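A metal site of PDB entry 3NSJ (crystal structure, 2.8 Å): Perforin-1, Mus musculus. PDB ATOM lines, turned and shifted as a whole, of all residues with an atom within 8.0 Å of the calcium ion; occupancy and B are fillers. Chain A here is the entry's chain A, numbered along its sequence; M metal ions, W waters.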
ATOM      1  N   THR A 411      -1.691 -27.843 -15.457  1.00  0.00           N
ATOM      2  CA  THR A 411      -2.687 -27.117 -14.692  1.00  0.00           C
ATOM      3  C   THR A 411      -3.770 -26.503 -15.579  1.00  0.00           C
ATOM      4  O   THR A 411      -3.596 -26.401 -16.799  1.00  0.00           O
ATOM      5  CB  THR A 411      -1.982 -26.055 -13.790  1.00  0.00           C
ATOM      6  OG1 THR A 411      -2.946 -25.297 -13.071  1.00  0.00           O
ATOM      7  CG2 THR A 411      -1.096 -25.098 -14.567  1.00  0.00           C
ATOM      8  N   ALA A 413      -4.611 -23.446 -14.886  1.00  0.00           N
ATOM      9  CA  ALA A 413      -4.186 -22.055 -14.818  1.00  0.00           C
ATOM     10  C   ALA A 413      -3.367 -21.735 -16.081  1.00  0.00           C
ATOM     11  O   ALA A 413      -2.202 -22.132 -16.200  1.00  0.00           O
ATOM     12  CB  ALA A 413      -3.344 -21.820 -13.581  1.00  0.00           C
ATOM     13  N   THR A 414      -4.014 -21.045 -17.043  1.00  0.00           N
ATOM     14  CA  THR A 414      -3.397 -20.718 -18.329  1.00  0.00           C
ATOM     15  C   THR A 414      -2.953 -19.267 -18.424  1.00  0.00           C
ATOM     16  O   THR A 414      -3.743 -18.355 -18.178  1.00  0.00           O
ATOM     17  CB  THR A 414      -4.309 -21.180 -19.458  1.00  0.00           C
ATOM     18  OG1 THR A 414      -4.584 -22.559 -19.267  1.00  0.00           O
ATOM     19  CG2 THR A 414      -3.687 -21.001 -20.830  1.00  0.00           C
ATOM     20  N   ASP A 415      -1.698 -19.058 -18.803  1.00  0.00           N
ATOM     21  CA  ASP A 415      -1.098 -17.748 -19.012  1.00  0.00           C
ATOM     22  C   ASP A 415      -0.694 -17.722 -20.489  1.00  0.00           C
ATOM     23  O   ASP A 415       0.493 -17.723 -20.827  1.00  0.00           O
ATOM     24  CB  ASP A 415       0.105 -17.545 -18.080  1.00  0.00           C
ATOM     25  CG  ASP A 415      -0.185 -17.925 -16.641  1.00  0.00           C
ATOM     26  OD1 ASP A 415       0.548 -18.761 -16.092  1.00  0.00           O
ATOM     27  OD2 ASP A 415      -1.168 -17.398 -16.077  1.00  0.00           O
ATOM     28  N   ALA A 416      -1.701 -17.764 -21.355  1.00  0.00           N
ATOM     29  CA  ALA A 416      -1.514 -17.857 -22.792  1.00  0.00           C
ATOM     30  C   ALA A 416      -1.060 -16.592 -23.495  1.00  0.00           C
ATOM     31  O   ALA A 416      -1.281 -15.474 -23.022  1.00  0.00           O
ATOM     32  CB  ALA A 416      -2.773 -18.395 -23.458  1.00  0.00           C
ATOM     33  N   TYR A 417      -0.410 -16.806 -24.641  1.00  0.00           N
ATOM     34  CA  TYR A 417       0.045 -15.838 -25.624  1.00  0.00           C
ATOM     35  C   TYR A 417       0.229 -16.577 -26.948  1.00  0.00           C
ATOM     36  O   TYR A 417       0.361 -17.809 -26.950  1.00  0.00           O
ATOM     37  CB  TYR A 417       1.285 -15.029 -25.174  1.00  0.00           C
ATOM     38  CG  TYR A 417       2.593 -15.802 -25.109  1.00  0.00           C
ATOM     39  CD1 TYR A 417       3.451 -15.841 -26.197  1.00  0.00           C
ATOM     40  CD2 TYR A 417       3.002 -16.404 -23.928  1.00  0.00           C
ATOM     41  CE1 TYR A 417       4.669 -16.519 -26.137  1.00  0.00           C
ATOM     42  CE2 TYR A 417       4.220 -17.086 -23.851  1.00  0.00           C
ATOM     43  CZ  TYR A 417       5.051 -17.127 -24.957  1.00  0.00           C
ATOM     44  OH  TYR A 417       6.249 -17.810 -24.911  1.00  0.00           O
ATOM     45  N   VAL A 431       0.811 -11.631 -22.841  1.00  0.00           N
ATOM     46  CA  VAL A 431       0.305 -12.705 -22.005  1.00  0.00           C
ATOM     47  C   VAL A 431      -1.008 -12.286 -21.356  1.00  0.00           C
ATOM     48  O   VAL A 431      -1.153 -11.130 -20.951  1.00  0.00           O
ATOM     49  CB  VAL A 431       1.353 -13.180 -20.951  1.00  0.00           C
ATOM     50  CG1 VAL A 431       0.841 -14.391 -20.174  1.00  0.00           C
ATOM     51  CG2 VAL A 431       2.690 -13.501 -21.598  1.00  0.00           C
ATOM     52  N   VAL A 432      -1.983 -13.220 -21.290  1.00  0.00           N
ATOM     53  CA  VAL A 432      -3.253 -13.032 -20.611  1.00  0.00           C
ATOM     54  C   VAL A 432      -3.142 -13.992 -19.434  1.00  0.00           C
ATOM     55  O   VAL A 432      -3.281 -15.196 -19.597  1.00  0.00           O
ATOM     56  CB  VAL A 432      -4.494 -13.310 -21.503  1.00  0.00           C
ATOM     57  CG1 VAL A 432      -5.787 -13.144 -20.705  1.00  0.00           C
ATOM     58  CG2 VAL A 432      -4.506 -12.400 -22.735  1.00  0.00           C
ATOM     59  N   TRP A 433      -2.793 -13.427 -18.274  1.00  0.00           N
ATOM     60  CA  TRP A 433      -2.550 -14.156 -17.037  1.00  0.00           C
ATOM     61  C   TRP A 433      -3.782 -14.802 -16.461  1.00  0.00           C
ATOM     62  O   TRP A 433      -4.837 -14.150 -16.372  1.00  0.00           O
ATOM     63  CB  TRP A 433      -1.835 -13.252 -16.014  1.00  0.00           C
ATOM     64  CG  TRP A 433      -0.552 -12.698 -16.542  1.00  0.00           C
ATOM     65  CD1 TRP A 433      -0.375 -11.508 -17.177  1.00  0.00           C
ATOM     66  CD2 TRP A 433       0.700 -13.391 -16.647  1.00  0.00           C
ATOM     67  NE1 TRP A 433       0.922 -11.380 -17.624  1.00  0.00           N
ATOM     68  CE2 TRP A 433       1.604 -12.525 -17.304  1.00  0.00           C
ATOM     69  CE3 TRP A 433       1.162 -14.656 -16.222  1.00  0.00           C
ATOM     70  CZ2 TRP A 433       2.943 -12.889 -17.545  1.00  0.00           C
ATOM     71  CZ3 TRP A 433       2.477 -15.013 -16.461  1.00  0.00           C
ATOM     72  CH2 TRP A 433       3.349 -14.129 -17.113  1.00  0.00           C
ATOM     73  N   ASN A 434      -3.663 -16.103 -16.093  1.00  0.00           N
ATOM     74  CA  ASN A 434      -4.690 -16.928 -15.456  1.00  0.00           C
ATOM     75  C   ASN A 434      -6.068 -16.782 -16.136  1.00  0.00           C
ATOM     76  O   ASN A 434      -6.964 -16.099 -15.604  1.00  0.00           O
ATOM     77  CB  ASN A 434      -4.740 -16.631 -13.948  1.00  0.00           C
ATOM     78  CG  ASN A 434      -5.311 -17.740 -13.096  1.00  0.00           C
ATOM     79  OD1 ASN A 434      -6.143 -18.541 -13.532  1.00  0.00           O
ATOM     80  ND2 ASN A 434      -4.889 -17.766 -11.838  1.00  0.00           N
ATOM     81  N   TRP A 462       1.275 -20.640 -26.708  1.00  0.00           N
ATOM     82  CA  TRP A 462       2.240 -20.846 -25.632  1.00  0.00           C
ATOM     83  C   TRP A 462       1.656 -20.551 -24.263  1.00  0.00           C
ATOM     84  O   TRP A 462       0.694 -19.790 -24.152  1.00  0.00           O
ATOM     85  CB  TRP A 462       3.491 -19.987 -25.867  1.00  0.00           C
ATOM     86  CG  TRP A 462       4.364 -20.463 -26.984  1.00  0.00           C
ATOM     87  CD1 TRP A 462       4.284 -20.111 -28.295  1.00  0.00           C
ATOM     88  CD2 TRP A 462       5.477 -21.356 -26.873  1.00  0.00           C
ATOM     89  NE1 TRP A 462       5.276 -20.746 -29.017  1.00  0.00           N
ATOM     90  CE2 TRP A 462       6.022 -21.510 -28.170  1.00  0.00           C
ATOM     91  CE3 TRP A 462       6.082 -22.044 -25.803  1.00  0.00           C
ATOM     92  CZ2 TRP A 462       7.115 -22.348 -28.426  1.00  0.00           C
ATOM     93  CZ3 TRP A 462       7.171 -22.865 -26.061  1.00  0.00           C
ATOM     94  CH2 TRP A 462       7.679 -23.014 -27.357  1.00  0.00           C
ATOM     95  N   ASP A 463       2.269 -21.127 -23.218  1.00  0.00           N
ATOM     96  CA  ASP A 463       1.881 -20.912 -21.833  1.00  0.00           C
ATOM     97  C   ASP A 463       3.083 -20.319 -21.093  1.00  0.00           C
ATOM     98  O   ASP A 463       4.087 -21.008 -20.912  1.00  0.00           O
ATOM     99  CB  ASP A 463       1.447 -22.232 -21.185  1.00  0.00           C
ATOM    100  CG  ASP A 463       0.594 -22.111 -19.940  1.00  0.00           C
ATOM    101  OD1 ASP A 463       0.025 -23.118 -19.515  1.00  0.00           O
ATOM    102  OD2 ASP A 463       0.498 -20.987 -19.393  1.00  0.00           O
ATOM    103  N   ALA A 464       2.984 -19.027 -20.712  1.00  0.00           N
ATOM    104  CA  ALA A 464       4.052 -18.288 -20.030  1.00  0.00           C
ATOM    105  C   ALA A 464       4.368 -18.867 -18.664  1.00  0.00           C
ATOM    106  O   ALA A 464       3.465 -19.044 -17.841  1.00  0.00           O
ATOM    107  CB  ALA A 464       3.688 -16.823 -19.902  1.00  0.00           C
ATOM    108  N   ASP A 465       5.649 -19.206 -18.451  1.00  0.00           N
ATOM    109  CA  ASP A 465       6.187 -19.780 -17.227  1.00  0.00           C
ATOM    110  C   ASP A 465       7.321 -18.873 -16.775  1.00  0.00           C
ATOM    111  O   ASP A 465       8.295 -18.711 -17.519  1.00  0.00           O
ATOM    112  CB  ASP A 465       6.695 -21.202 -17.504  1.00  0.00           C
ATOM    113  CG  ASP A 465       6.760 -22.148 -16.323  1.00  0.00           C
ATOM    114  OD1 ASP A 465       6.511 -21.693 -15.186  1.00  0.00           O
ATOM    115  OD2 ASP A 465       7.048 -23.347 -16.543  1.00  0.00           O
ATOM    116  N   TYR A 466       7.169 -18.225 -15.594  1.00  0.00           N
ATOM    117  CA  TYR A 466       8.117 -17.247 -15.018  1.00  0.00           C
ATOM    118  C   TYR A 466       9.614 -17.565 -15.145  1.00  0.00           C
ATOM    119  O   TYR A 466      10.259 -17.069 -16.077  1.00  0.00           O
ATOM    120  CB  TYR A 466       7.723 -16.868 -13.573  1.00  0.00           C
ATOM    121  N   ASP A 470       8.895 -21.588 -21.166  1.00  0.00           N
ATOM    122  CA  ASP A 470       7.466 -21.576 -21.469  1.00  0.00           C
ATOM    123  C   ASP A 470       7.044 -22.849 -22.175  1.00  0.00           C
ATOM    124  O   ASP A 470       7.832 -23.392 -22.952  1.00  0.00           O
ATOM    125  CB  ASP A 470       7.119 -20.368 -22.362  1.00  0.00           C
ATOM    126  CG  ASP A 470       7.318 -19.007 -21.724  1.00  0.00           C
ATOM    127  OD1 ASP A 470       7.817 -18.953 -20.582  1.00  0.00           O
ATOM    128  OD2 ASP A 470       6.968 -18.001 -22.371  1.00  0.00           O
ATOM    129  N   ASP A 471       5.828 -23.344 -21.906  1.00  0.00           N
ATOM    130  CA  ASP A 471       5.379 -24.557 -22.602  1.00  0.00           C
ATOM    131  C   ASP A 471       4.390 -24.320 -23.735  1.00  0.00           C
ATOM    132  O   ASP A 471       3.467 -23.505 -23.622  1.00  0.00           O
ATOM    133  CB  ASP A 471       4.991 -25.705 -21.665  1.00  0.00           C
ATOM    134  CG  ASP A 471       3.715 -25.513 -20.872  1.00  0.00           C
ATOM    135  OD1 ASP A 471       2.643 -25.952 -21.370  1.00  0.00           O
ATOM    136  OD2 ASP A 471       3.790 -25.020 -19.725  1.00  0.00           O
ATOM    137  N   LEU A 473       1.379 -25.116 -25.813  1.00  0.00           N
ATOM    138  CA  LEU A 473       0.077 -25.751 -25.604  1.00  0.00           C
ATOM    139  C   LEU A 473      -0.426 -26.419 -26.869  1.00  0.00           C
ATOM    140  O   LEU A 473      -1.240 -27.334 -26.798  1.00  0.00           O
ATOM    141  CB  LEU A 473      -0.962 -24.728 -25.121  1.00  0.00           C
ATOM    142  CG  LEU A 473      -0.671 -24.020 -23.817  1.00  0.00           C
ATOM    143  CD1 LEU A 473      -1.812 -23.105 -23.463  1.00  0.00           C
ATOM    144  CD2 LEU A 473      -0.431 -24.996 -22.691  1.00  0.00           C
HETATM  145 CA    CA M   1       1.623 -20.560 -17.253  1.00  0.00          CA
HETATM  146  O   HOH W   1       0.664 -23.035 -16.588  1.00  0.00           O
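Water W1 lies within hydrogen-bond range of OD1 of Asp 463 (3.0 Å) and O of Ala 413 (3.0 Å).
OD2 of Asp 415 lies within hydrogen-bond range of N of Asn 434. N of Asp 463 lies within hydrogen-bond range of O of Asp 471 (2.7 Å).
Three residues have an atom within 4 Å of the calcium ion: Asp 415, Asp 463 and Ala 464.
The calcium ion is bound by OD1 of Asp 415 (2.4 Å). The calcium ion is bound by OD2 of Asp 463 (2.5 Å). The calcium ion is bound by O of Ala 464 (2.5 Å). The calcium ion is bound by water W1 (2.7 Å). The calcium ion has four donor atoms within binding distance.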
